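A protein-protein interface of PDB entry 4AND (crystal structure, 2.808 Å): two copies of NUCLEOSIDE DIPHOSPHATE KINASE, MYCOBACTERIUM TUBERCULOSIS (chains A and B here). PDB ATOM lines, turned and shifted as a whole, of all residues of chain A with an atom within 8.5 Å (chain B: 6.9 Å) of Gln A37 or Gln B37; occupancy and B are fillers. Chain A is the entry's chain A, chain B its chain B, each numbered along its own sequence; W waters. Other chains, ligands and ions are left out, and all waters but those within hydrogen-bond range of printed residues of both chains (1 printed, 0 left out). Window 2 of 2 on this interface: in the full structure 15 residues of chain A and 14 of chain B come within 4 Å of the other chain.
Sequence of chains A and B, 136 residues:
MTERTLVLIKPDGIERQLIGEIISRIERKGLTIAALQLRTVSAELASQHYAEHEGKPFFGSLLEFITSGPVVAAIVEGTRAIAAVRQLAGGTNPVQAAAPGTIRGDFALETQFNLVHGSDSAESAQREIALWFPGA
The backbone NH (N) of Leu A38 is in hydrogen-bond range of the backbone carbonyl oxygen (O) of Leu B36 (2.8 Å). The backbone NH (N) of Leu B38 lies within hydrogen-bond range of the backbone carbonyl oxygen (O) of Leu A36, 2.8 Å away.
N of Ala A34 sits at hydrogen-bond distance from O of Ile A75, 2.8 Å away. N of Ile A75 sits at hydrogen-bond distance from O of Ala A35, at 2.9 Å. N of Ala B73 lies within hydrogen-bond range of O of Gln B37 (2.8 Å). The backbone carbonyl oxygen (O) of Gln A37 sits at hydrogen-bond distance from the backbone NH (N) of Ala A73.
Ile A33 touches Leu B38 (O to CD2, 3.5 Å). Leu B38 touches Ala A34. CA of Ala A35 touches CD2 of Leu B38 (3.97 Å). Leu A36 touches Leu B36 (O to O, 3.99 Å). Leu A36 touches Gln B37. Leu B36 touches Gln A37. Gln A37 touches Gln B37. CD2 of Leu A38 touches O of Ile B33, at 3.6 Å.
Printed residues of chain B within 4 Å of Ile A33: Leu B38 (3.5 Å). Of the printed residues of chain B, Gln A37 touches Leu B36 (3.2 Å) and Gln B37 (3.8 Å). Of the printed residues of chain B, Leu A38 touches Ile B33 (3.6 Å) and Leu B36 (2.8 Å). Val A71 touches none of the printed residues of chain B. Of the printed residues of chain A, Leu B38 touches Ile A33, Ala A34, Ala A35 and Leu A36.
Printed residues of chain A that touch a printed residue of chain B: Ile A33, Ala A34, Ala A35, Leu A36, Gln A37 and Leu A38. Among the printed residues, 10 pairs touch across the chains.
Ala A35 touches Leu B38, but with the chains exchanged Leu A38 does not touch Ala B35 (4.02 Å). Leu A36 touches its own counterpart, Leu B36. Leu A36 touches Gln B37, and with the chains exchanged Gln A37 touches Leu B36. Gln B37 touches its own counterpart, Gln A37. Positions printed for both chains: 33, 35, 36, 37, 38, 39, 71, 72, 73, 74, 75, 132 and 133. Of the 10 pairs that touch across the chains among the printed residues, 8 have their exchanged pair printed and touching as well.
Water W1 lies within hydrogen-bond range of the backbone carbonyl oxygen of Leu B38 (2.8 Å) and the backbone NH of Leu A36 (2.8 Å).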
ATOM      1  N   VAL A   7     -24.924  15.001  16.649  1.00  0.00           N
ATOM      2  CA  VAL A   7     -23.952  14.236  17.402  1.00  0.00           C
ATOM      3  C   VAL A   7     -23.458  13.071  16.564  1.00  0.00           C
ATOM      4  O   VAL A   7     -24.250  12.373  15.931  1.00  0.00           O
ATOM      5  CB  VAL A   7     -24.548  13.709  18.722  1.00  0.00           C
ATOM      6  CG1 VAL A   7     -23.565  12.778  19.415  1.00  0.00           C
ATOM      7  CG2 VAL A   7     -24.924  14.875  19.628  1.00  0.00           C
ATOM      8  N   LEU A   8     -22.144  12.878  16.544  1.00  0.00           N
ATOM      9  CA  LEU A   8     -21.556  11.727  15.874  1.00  0.00           C
ATOM     10  C   LEU A   8     -20.791  10.890  16.882  1.00  0.00           C
ATOM     11  O   LEU A   8     -20.061  11.431  17.719  1.00  0.00           O
ATOM     12  CB  LEU A   8     -20.594  12.172  14.773  1.00  0.00           C
ATOM     13  CG  LEU A   8     -21.135  13.035  13.641  1.00  0.00           C
ATOM     14  CD1 LEU A   8     -19.985  13.523  12.787  1.00  0.00           C
ATOM     15  CD2 LEU A   8     -22.139  12.252  12.818  1.00  0.00           C
ATOM     16  N   ILE A   9     -20.967   9.574  16.810  1.00  0.00           N
ATOM     17  CA  ILE A   9     -20.094   8.659  17.526  1.00  0.00           C
ATOM     18  C   ILE A   9     -19.148   8.069  16.494  1.00  0.00           C
ATOM     19  O   ILE A   9     -19.523   7.189  15.716  1.00  0.00           O
ATOM     20  CB  ILE A   9     -20.873   7.548  18.238  1.00  0.00           C
ATOM     21  CG1 ILE A   9     -21.901   8.154  19.193  1.00  0.00           C
ATOM     22  CG2 ILE A   9     -19.921   6.639  18.999  1.00  0.00           C
ATOM     23  CD1 ILE A   9     -22.741   7.131  19.912  1.00  0.00           C
ATOM     24  N   ILE A  14     -17.057   3.510  18.490  1.00  0.00           N
ATOM     25  CA  ILE A  14     -17.750   2.254  18.228  1.00  0.00           C
ATOM     26  C   ILE A  14     -16.875   1.036  18.519  1.00  0.00           C
ATOM     27  O   ILE A  14     -17.327   0.073  19.149  1.00  0.00           O
ATOM     28  CB  ILE A  14     -18.256   2.192  16.779  1.00  0.00           C
ATOM     29  CG1 ILE A  14     -19.341   3.253  16.563  1.00  0.00           C
ATOM     30  CG2 ILE A  14     -18.774   0.798  16.456  1.00  0.00           C
ATOM     31  CD1 ILE A  14     -19.914   3.280  15.170  1.00  0.00           C
ATOM     32  N   ILE A  23     -24.897   7.376  24.463  1.00  0.00           N
ATOM     33  CA  ILE A  23     -26.326   7.647  24.414  1.00  0.00           C
ATOM     34  C   ILE A  23     -26.896   7.792  25.832  1.00  0.00           C
ATOM     35  O   ILE A  23     -27.628   8.746  26.124  1.00  0.00           O
ATOM     36  CB  ILE A  23     -27.076   6.568  23.612  1.00  0.00           C
ATOM     37  CG1 ILE A  23     -26.556   6.541  22.170  1.00  0.00           C
ATOM     38  CG2 ILE A  23     -28.580   6.823  23.649  1.00  0.00           C
ATOM     39  CD1 ILE A  23     -27.236   5.525  21.286  1.00  0.00           C
ATOM     40  N   ILE A  33     -33.230  11.621  22.083  1.00  0.00           N
ATOM     41  CA  ILE A  33     -32.738  11.219  20.776  1.00  0.00           C
ATOM     42  C   ILE A  33     -33.850  11.397  19.747  1.00  0.00           C
ATOM     43  O   ILE A  33     -34.778  10.588  19.678  1.00  0.00           O
ATOM     44  CB  ILE A  33     -32.280   9.744  20.772  1.00  0.00           C
ATOM     45  CG1 ILE A  33     -31.459   9.431  22.024  1.00  0.00           C
ATOM     46  CG2 ILE A  33     -31.466   9.432  19.517  1.00  0.00           C
ATOM     47  CD1 ILE A  33     -30.104  10.119  22.047  1.00  0.00           C
ATOM     48  N   ALA A  34     -33.757  12.465  18.960  1.00  0.00           N
ATOM     49  CA  ALA A  34     -34.761  12.771  17.942  1.00  0.00           C
ATOM     50  C   ALA A  34     -34.554  11.940  16.680  1.00  0.00           C
ATOM     51  O   ALA A  34     -35.513  11.566  16.008  1.00  0.00           O
ATOM     52  CB  ALA A  34     -34.743  14.258  17.607  1.00  0.00           C
ATOM     53  N   ALA A  35     -33.294  11.658  16.364  1.00  0.00           N
ATOM     54  CA  ALA A  35     -32.954  10.819  15.220  1.00  0.00           C
ATOM     55  C   ALA A  35     -31.710  10.016  15.555  1.00  0.00           C
ATOM     56  O   ALA A  35     -30.872  10.468  16.328  1.00  0.00           O
ATOM     57  CB  ALA A  35     -32.722  11.663  13.983  1.00  0.00           C
ATOM     58  N   LEU A  36     -31.588   8.830  14.967  1.00  0.00           N
ATOM     59  CA  LEU A  36     -30.484   7.933  15.288  1.00  0.00           C
ATOM     60  C   LEU A  36     -30.263   6.903  14.186  1.00  0.00           C
ATOM     61  O   LEU A  36     -31.186   6.183  13.801  1.00  0.00           O
ATOM     62  CB  LEU A  36     -30.755   7.218  16.611  1.00  0.00           C
ATOM     63  CG  LEU A  36     -29.681   6.233  17.075  1.00  0.00           C
ATOM     64  CD1 LEU A  36     -28.406   6.970  17.471  1.00  0.00           C
ATOM     65  CD2 LEU A  36     -30.201   5.398  18.232  1.00  0.00           C
ATOM     66  N   GLN A  37     -29.030   6.827  13.692  1.00  0.00           N
ATOM     67  CA  GLN A  37     -28.713   5.929  12.590  1.00  0.00           C
ATOM     68  C   GLN A  37     -27.226   5.598  12.489  1.00  0.00           C
ATOM     69  O   GLN A  37     -26.376   6.486  12.484  1.00  0.00           O
ATOM     70  CB  GLN A  37     -29.198   6.527  11.268  1.00  0.00           C
ATOM     71  CG  GLN A  37     -28.972   5.621  10.079  1.00  0.00           C
ATOM     72  CD  GLN A  37     -29.211   6.324   8.766  1.00  0.00           C
ATOM     73  OE1 GLN A  37     -28.902   7.507   8.617  1.00  0.00           O
ATOM     74  NE2 GLN A  37     -29.765   5.600   7.803  1.00  0.00           N
ATOM     75  N   LEU A  38     -26.924   4.306  12.417  1.00  0.00           N
ATOM     76  CA  LEU A  38     -25.585   3.842  12.082  1.00  0.00           C
ATOM     77  C   LEU A  38     -25.490   3.797  10.563  1.00  0.00           C
ATOM     78  O   LEU A  38     -26.307   3.153   9.903  1.00  0.00           O
ATOM     79  CB  LEU A  38     -25.332   2.448  12.658  1.00  0.00           C
ATOM     80  CG  LEU A  38     -24.014   1.779  12.254  1.00  0.00           C
ATOM     81  CD1 LEU A  38     -22.847   2.407  13.003  1.00  0.00           C
ATOM     82  CD2 LEU A  38     -24.057   0.280  12.489  1.00  0.00           C
ATOM     83  N   ARG A  39     -24.495   4.484  10.012  1.00  0.00           N
ATOM     84  CA  ARG A  39     -24.390   4.661   8.572  1.00  0.00           C
ATOM     85  C   ARG A  39     -22.937   4.767   8.139  1.00  0.00           C
ATOM     86  O   ARG A  39     -22.045   4.925   8.968  1.00  0.00           O
ATOM     87  CB  ARG A  39     -25.125   5.932   8.159  1.00  0.00           C
ATOM     88  CG  ARG A  39     -24.704   7.158   8.945  1.00  0.00           C
ATOM     89  CD  ARG A  39     -25.205   8.424   8.286  1.00  0.00           C
ATOM     90  NE  ARG A  39     -24.646   8.567   6.947  1.00  0.00           N
ATOM     91  CZ  ARG A  39     -24.987   9.523   6.090  1.00  0.00           C
ATOM     92  NH1 ARG A  39     -25.894  10.429   6.427  1.00  0.00           N
ATOM     93  NH2 ARG A  39     -24.423   9.568   4.891  1.00  0.00           N
ATOM     94  N   THR A  40     -22.697   4.682   6.836  1.00  0.00           N
ATOM     95  CA  THR A  40     -21.361   4.926   6.304  1.00  0.00           C
ATOM     96  C   THR A  40     -21.259   6.361   5.802  1.00  0.00           C
ATOM     97  O   THR A  40     -22.271   7.013   5.548  1.00  0.00           O
ATOM     98  CB  THR A  40     -20.994   3.947   5.174  1.00  0.00           C
ATOM     99  OG1 THR A  40     -22.035   3.938   4.189  1.00  0.00           O
ATOM    100  CG2 THR A  40     -20.810   2.543   5.733  1.00  0.00           C
ATOM    101  N   LEU A  45     -19.501  13.583   1.723  1.00  0.00           N
ATOM    102  CA  LEU A  45     -20.168  13.918   2.977  1.00  0.00           C
ATOM    103  C   LEU A  45     -19.124  14.259   4.027  1.00  0.00           C
ATOM    104  O   LEU A  45     -19.310  15.171   4.833  1.00  0.00           O
ATOM    105  CB  LEU A  45     -21.032  12.757   3.469  1.00  0.00           C
ATOM    106  CG  LEU A  45     -21.553  12.867   4.905  1.00  0.00           C
ATOM    107  CD1 LEU A  45     -22.361  14.142   5.103  1.00  0.00           C
ATOM    108  CD2 LEU A  45     -22.378  11.648   5.279  1.00  0.00           C
ATOM    109  N   PRO A  70     -18.189   2.703   9.744  1.00  0.00           N
ATOM    110  CA  PRO A  70     -19.455   3.425   9.868  1.00  0.00           C
ATOM    111  C   PRO A  70     -19.481   4.213  11.168  1.00  0.00           C
ATOM    112  O   PRO A  70     -18.757   3.878  12.106  1.00  0.00           O
ATOM    113  CB  PRO A  70     -20.485   2.300   9.912  1.00  0.00           C
ATOM    114  CG  PRO A  70     -19.756   1.180  10.571  1.00  0.00           C
ATOM    115  CD  PRO A  70     -18.335   1.274  10.074  1.00  0.00           C
ATOM    116  N   VAL A  71     -20.298   5.257  11.215  1.00  0.00           N
ATOM    117  CA  VAL A  71     -20.443   6.053  12.421  1.00  0.00           C
ATOM    118  C   VAL A  71     -21.896   6.026  12.861  1.00  0.00           C
ATOM    119  O   VAL A  71     -22.770   5.594  12.114  1.00  0.00           O
ATOM    120  CB  VAL A  71     -20.018   7.513  12.187  1.00  0.00           C
ATOM    121  CG1 VAL A  71     -18.655   7.569  11.508  1.00  0.00           C
ATOM    122  CG2 VAL A  71     -21.058   8.235  11.352  1.00  0.00           C
ATOM    123  N   VAL A  72     -22.153   6.472  14.085  1.00  0.00           N
ATOM    124  CA  VAL A  72     -23.524   6.631  14.545  1.00  0.00           C
ATOM    125  C   VAL A  72     -23.868   8.108  14.553  1.00  0.00           C
ATOM    126  O   VAL A  72     -23.298   8.883  15.317  1.00  0.00           O
ATOM    127  CB  VAL A  72     -23.751   6.027  15.941  1.00  0.00           C
ATOM    128  CG1 VAL A  72     -25.174   6.285  16.404  1.00  0.00           C
ATOM    129  CG2 VAL A  72     -23.473   4.537  15.924  1.00  0.00           C
ATOM    130  N   ALA A  73     -24.782   8.498  13.674  1.00  0.00           N
ATOM    131  CA  ALA A  73     -25.238   9.876  13.623  1.00  0.00           C
ATOM    132  C   ALA A  73     -26.543  10.000  14.390  1.00  0.00           C
ATOM    133  O   ALA A  73     -27.357   9.076  14.401  1.00  0.00           O
ATOM    134  CB  ALA A  73     -25.411  10.328  12.191  1.00  0.00           C
ATOM    135  N   ALA A  74     -26.738  11.142  15.037  1.00  0.00           N
ATOM    136  CA  ALA A  74     -27.921  11.341  15.853  1.00  0.00           C
ATOM    137  C   ALA A  74     -28.304  12.809  15.921  1.00  0.00           C
ATOM    138  O   ALA A  74     -27.441  13.685  15.911  1.00  0.00           O
ATOM    139  CB  ALA A  74     -27.694  10.786  17.252  1.00  0.00           C
ATOM    140  N   ILE A  75     -29.604  13.074  15.976  1.00  0.00           N
ATOM    141  CA  ILE A  75     -30.087  14.411  16.273  1.00  0.00           C
ATOM    142  C   ILE A  75     -30.499  14.443  17.736  1.00  0.00           C
ATOM    143  O   ILE A  75     -31.396  13.708  18.150  1.00  0.00           O
ATOM    144  CB  ILE A  75     -31.294  14.798  15.393  1.00  0.00           C
ATOM    145  CG1 ILE A  75     -30.859  14.956  13.937  1.00  0.00           C
ATOM    146  CG2 ILE A  75     -31.937  16.088  15.893  1.00  0.00           C
ATOM    147  CD1 ILE A  75     -31.969  15.389  13.012  1.00  0.00           C
ATOM    148  N   LEU A 131     -26.847  18.045   6.224  1.00  0.00           N
ATOM    149  CA  LEU A 131     -26.002  17.090   5.511  1.00  0.00           C
ATOM    150  C   LEU A 131     -26.256  15.650   5.952  1.00  0.00           C
ATOM    151  O   LEU A 131     -26.331  14.741   5.127  1.00  0.00           O
ATOM    152  CB  LEU A 131     -24.522  17.426   5.719  1.00  0.00           C
ATOM    153  CG  LEU A 131     -24.078  18.880   5.541  1.00  0.00           C
ATOM    154  CD1 LEU A 131     -22.594  19.029   5.861  1.00  0.00           C
ATOM    155  CD2 LEU A 131     -24.385  19.381   4.134  1.00  0.00           C
ATOM    156  N   TRP A 132     -26.382  15.451   7.260  1.00  0.00           N
ATOM    157  CA  TRP A 132     -26.480  14.112   7.837  1.00  0.00           C
ATOM    158  C   TRP A 132     -27.904  13.557   7.859  1.00  0.00           C
ATOM    159  O   TRP A 132     -28.106  12.343   7.814  1.00  0.00           O
ATOM    160  CB  TRP A 132     -25.876  14.100   9.244  1.00  0.00           C
ATOM    161  CG  TRP A 132     -24.384  14.204   9.258  1.00  0.00           C
ATOM    162  CD1 TRP A 132     -23.635  15.349   9.260  1.00  0.00           C
ATOM    163  CD2 TRP A 132     -23.452  13.116   9.270  1.00  0.00           C
ATOM    164  NE1 TRP A 132     -22.289  15.037   9.275  1.00  0.00           N
ATOM    165  CE2 TRP A 132     -22.155  13.674   9.281  1.00  0.00           C
ATOM    166  CE3 TRP A 132     -23.590  11.726   9.273  1.00  0.00           C
ATOM    167  CZ2 TRP A 132     -21.012  12.888   9.296  1.00  0.00           C
ATOM    168  CZ3 TRP A 132     -22.450  10.950   9.288  1.00  0.00           C
ATOM    169  CH2 TRP A 132     -21.179  11.532   9.300  1.00  0.00           C
ATOM    170  N   PHE A 133     -28.886  14.447   7.937  1.00  0.00           N
ATOM    171  CA  PHE A 133     -30.289  14.048   7.922  1.00  0.00           C
ATOM    172  C   PHE A 133     -31.088  14.932   6.967  1.00  0.00           C
ATOM    173  O   PHE A 133     -31.896  15.749   7.404  1.00  0.00           O
ATOM    174  CB  PHE A 133     -30.887  14.104   9.335  1.00  0.00           C
ATOM    175  CG  PHE A 133     -30.331  13.067  10.272  1.00  0.00           C
ATOM    176  CD1 PHE A 133     -29.179  13.318  11.006  1.00  0.00           C
ATOM    177  CD2 PHE A 133     -30.954  11.838  10.414  1.00  0.00           C
ATOM    178  CE1 PHE A 133     -28.659  12.362  11.862  1.00  0.00           C
ATOM    179  CE2 PHE A 133     -30.441  10.878  11.271  1.00  0.00           C
ATOM    180  CZ  PHE A 133     -29.294  11.141  11.993  1.00  0.00           C
ATOM    181  N   PRO A 134     -30.858  14.764   5.654  1.00  0.00           N
ATOM    182  CA  PRO A 134     -31.448  15.600   4.602  1.00  0.00           C
ATOM    183  C   PRO A 134     -32.930  15.896   4.818  1.00  0.00           C
ATOM    184  O   PRO A 134     -33.318  17.061   4.843  1.00  0.00           O
ATOM    185  CB  PRO A 134     -31.255  14.751   3.348  1.00  0.00           C
ATOM    186  CG  PRO A 134     -30.012  13.985   3.622  1.00  0.00           C
ATOM    187  CD  PRO A 134     -30.035  13.677   5.094  1.00  0.00           C
ATOM    188  N   ILE B  33     -23.212  -4.105  17.172  1.00  0.00           N
ATOM    189  CA  ILE B  33     -24.341  -3.466  16.514  1.00  0.00           C
ATOM    190  C   ILE B  33     -24.056  -3.369  15.021  1.00  0.00           C
ATOM    191  O   ILE B  33     -23.279  -2.519  14.585  1.00  0.00           O
ATOM    192  CB  ILE B  33     -24.585  -2.046  17.066  1.00  0.00           C
ATOM    193  CG1 ILE B  33     -24.511  -2.042  18.595  1.00  0.00           C
ATOM    194  CG2 ILE B  33     -25.917  -1.495  16.569  1.00  0.00           C
ATOM    195  CD1 ILE B  33     -25.548  -2.918  19.260  1.00  0.00           C
ATOM    196  N   ALA B  35     -26.501  -2.973  12.624  1.00  0.00           N
ATOM    197  CA  ALA B  35     -27.380  -1.938  12.091  1.00  0.00           C
ATOM    198  C   ALA B  35     -28.131  -1.284  13.239  1.00  0.00           C
ATOM    199  O   ALA B  35     -28.401  -1.926  14.254  1.00  0.00           O
ATOM    200  CB  ALA B  35     -28.350  -2.529  11.091  1.00  0.00           C
ATOM    201  N   LEU B  36     -28.474  -0.009  13.081  1.00  0.00           N
ATOM    202  CA  LEU B  36     -29.114   0.742  14.155  1.00  0.00           C
ATOM    203  C   LEU B  36     -29.860   1.955  13.617  1.00  0.00           C
ATOM    204  O   LEU B  36     -29.282   2.790  12.921  1.00  0.00           O
ATOM    205  CB  LEU B  36     -28.069   1.185  15.184  1.00  0.00           C
ATOM    206  CG  LEU B  36     -28.512   2.092  16.338  1.00  0.00           C
ATOM    207  CD1 LEU B  36     -29.467   1.359  17.275  1.00  0.00           C
ATOM    208  CD2 LEU B  36     -27.305   2.626  17.104  1.00  0.00           C
ATOM    209  N   GLN B  37     -31.142   2.057  13.953  1.00  0.00           N
ATOM    210  CA  GLN B  37     -31.968   3.148  13.454  1.00  0.00           C
ATOM    211  C   GLN B  37     -33.204   3.415  14.318  1.00  0.00           C
ATOM    212  O   GLN B  37     -33.964   2.496  14.635  1.00  0.00           O
ATOM    213  CB  GLN B  37     -32.396   2.854  12.018  1.00  0.00           C
ATOM    214  CG  GLN B  37     -33.176   3.966  11.359  1.00  0.00           C
ATOM    215  CD  GLN B  37     -33.605   3.605   9.957  1.00  0.00           C
ATOM    216  OE1 GLN B  37     -34.257   2.583   9.739  1.00  0.00           O
ATOM    217  NE2 GLN B  37     -33.230   4.435   8.993  1.00  0.00           N
ATOM    218  N   LEU B  38     -33.389   4.676  14.698  1.00  0.00           N
ATOM    219  CA  LEU B  38     -34.637   5.118  15.304  1.00  0.00           C
ATOM    220  C   LEU B  38     -35.590   5.459  14.174  1.00  0.00           C
ATOM    221  O   LEU B  38     -35.262   6.263  13.303  1.00  0.00           O
ATOM    222  CB  LEU B  38     -34.420   6.353  16.178  1.00  0.00           C
ATOM    223  CG  LEU B  38     -35.702   6.951  16.770  1.00  0.00           C
ATOM    224  CD1 LEU B  38     -36.120   6.198  18.020  1.00  0.00           C
ATOM    225  CD2 LEU B  38     -35.508   8.421  17.080  1.00  0.00           C
ATOM    226  N   ARG B  39     -36.768   4.846  14.191  1.00  0.00           N
ATOM    227  CA  ARG B  39     -37.707   4.958  13.080  1.00  0.00           C
ATOM    228  C   ARG B  39     -39.145   4.859  13.570  1.00  0.00           C
ATOM    229  O   ARG B  39     -39.397   4.469  14.708  1.00  0.00           O
ATOM    230  CB  ARG B  39     -37.451   3.827  12.090  1.00  0.00           C
ATOM    231  CG  ARG B  39     -37.924   2.482  12.610  1.00  0.00           C
ATOM    232  CD  ARG B  39     -37.165   1.324  11.993  1.00  0.00           C
ATOM    233  NE  ARG B  39     -37.410   1.189  10.562  1.00  0.00           N
ATOM    234  CZ  ARG B  39     -38.509   0.653  10.041  1.00  0.00           C
ATOM    235  NH1 ARG B  39     -39.473   0.215  10.838  1.00  0.00           N
ATOM    236  NH2 ARG B  39     -38.648   0.564   8.726  1.00  0.00           N
ATOM    237  N   VAL B  71     -39.529   3.624  17.434  1.00  0.00           N
ATOM    238  CA  VAL B  71     -38.764   2.617  18.147  1.00  0.00           C
ATOM    239  C   VAL B  71     -37.328   2.624  17.650  1.00  0.00           C
ATOM    240  O   VAL B  71     -37.016   3.239  16.634  1.00  0.00           O
ATOM    241  CB  VAL B  71     -39.356   1.214  17.954  1.00  0.00           C
ATOM    242  CG1 VAL B  71     -40.852   1.250  18.201  1.00  0.00           C
ATOM    243  CG2 VAL B  71     -39.051   0.692  16.567  1.00  0.00           C
ATOM    244  N   VAL B  72     -36.448   1.952  18.377  1.00  0.00           N
ATOM    245  CA  VAL B  72     -35.082   1.781  17.909  1.00  0.00           C
ATOM    246  C   VAL B  72     -34.905   0.353  17.418  1.00  0.00           C
ATOM    247  O   VAL B  72     -34.979  -0.594  18.195  1.00  0.00           O
ATOM    248  CB  VAL B  72     -34.045   2.093  19.001  1.00  0.00           C
ATOM    249  CG1 VAL B  72     -32.642   1.871  18.462  1.00  0.00           C
ATOM    250  CG2 VAL B  72     -34.206   3.523  19.484  1.00  0.00           C
ATOM    251  N   ALA B  73     -34.696   0.201  16.117  1.00  0.00           N
ATOM    252  CA  ALA B  73     -34.471  -1.110  15.543  1.00  0.00           C
ATOM    253  C   ALA B  73     -32.981  -1.326  15.365  1.00  0.00           C
ATOM    254  O   ALA B  73     -32.243  -0.390  15.072  1.00  0.00           O
ATOM    255  CB  ALA B  73     -35.195  -1.240  14.218  1.00  0.00           C
ATOM    256  N   ALA B  74     -32.536  -2.563  15.533  1.00  0.00           N
ATOM    257  CA  ALA B  74     -31.118  -2.859  15.433  1.00  0.00           C
ATOM    258  C   ALA B  74     -30.876  -4.288  14.983  1.00  0.00           C
ATOM    259  O   ALA B  74     -31.640  -5.193  15.311  1.00  0.00           O
ATOM    260  CB  ALA B  74     -30.434  -2.605  16.774  1.00  0.00           C
ATOM    261  N   ILE B  75     -29.813  -4.483  14.215  1.00  0.00           N
ATOM    262  CA  ILE B  75     -29.350  -5.822  13.899  1.00  0.00           C
ATOM    263  C   ILE B  75     -28.165  -6.134  14.801  1.00  0.00           C
ATOM    264  O   ILE B  75     -27.142  -5.451  14.748  1.00  0.00           O
ATOM    265  CB  ILE B  75     -28.920  -5.950  12.423  1.00  0.00           C
ATOM    266  CG1 ILE B  75     -30.114  -5.730  11.499  1.00  0.00           C
ATOM    267  CG2 ILE B  75     -28.300  -7.315  12.161  1.00  0.00           C
ATOM    268  CD1 ILE B  75     -29.799  -5.964  10.039  1.00  0.00           C
ATOM    269  N   TRP B 132     -37.692  -5.208   8.778  1.00  0.00           N
ATOM    270  CA  TRP B 132     -37.178  -4.010   9.434  1.00  0.00           C
ATOM    271  C   TRP B 132     -35.968  -3.399   8.725  1.00  0.00           C
ATOM    272  O   TRP B 132     -35.736  -2.192   8.813  1.00  0.00           O
ATOM    273  CB  TRP B 132     -36.840  -4.309  10.895  1.00  0.00           C
ATOM    274  CG  TRP B 132     -38.037  -4.607  11.756  1.00  0.00           C
ATOM    275  CD1 TRP B 132     -38.639  -5.819  11.935  1.00  0.00           C
ATOM    276  CD2 TRP B 132     -38.763  -3.677  12.565  1.00  0.00           C
ATOM    277  NE1 TRP B 132     -39.696  -5.701  12.799  1.00  0.00           N
ATOM    278  CE2 TRP B 132     -39.794  -4.395  13.202  1.00  0.00           C
ATOM    279  CE3 TRP B 132     -38.643  -2.303  12.813  1.00  0.00           C
ATOM    280  CZ2 TRP B 132     -40.701  -3.790  14.068  1.00  0.00           C
ATOM    281  CZ3 TRP B 132     -39.542  -1.705  13.676  1.00  0.00           C
ATOM    282  CH2 TRP B 132     -40.557  -2.446  14.292  1.00  0.00           C
ATOM    283  N   PHE B 133     -35.196  -4.232   8.036  1.00  0.00           N
ATOM    284  CA  PHE B 133     -34.042  -3.759   7.278  1.00  0.00           C
ATOM    285  C   PHE B 133     -34.017  -4.386   5.886  1.00  0.00           C
ATOM    286  O   PHE B 133     -33.167  -5.226   5.594  1.00  0.00           O
ATOM    287  CB  PHE B 133     -32.738  -4.064   8.023  1.00  0.00           C
ATOM    288  CG  PHE B 133     -32.574  -3.295   9.301  1.00  0.00           C
ATOM    289  CD1 PHE B 133     -31.980  -2.043   9.300  1.00  0.00           C
ATOM    290  CD2 PHE B 133     -33.010  -3.825  10.506  1.00  0.00           C
ATOM    291  CE1 PHE B 133     -31.828  -1.332  10.476  1.00  0.00           C
ATOM    292  CE2 PHE B 133     -32.862  -3.122  11.682  1.00  0.00           C
ATOM    293  CZ  PHE B 133     -32.268  -1.872  11.668  1.00  0.00           C
HETATM  294  O   HOH W   1     -33.586   8.478  12.978  1.00  0.00           O
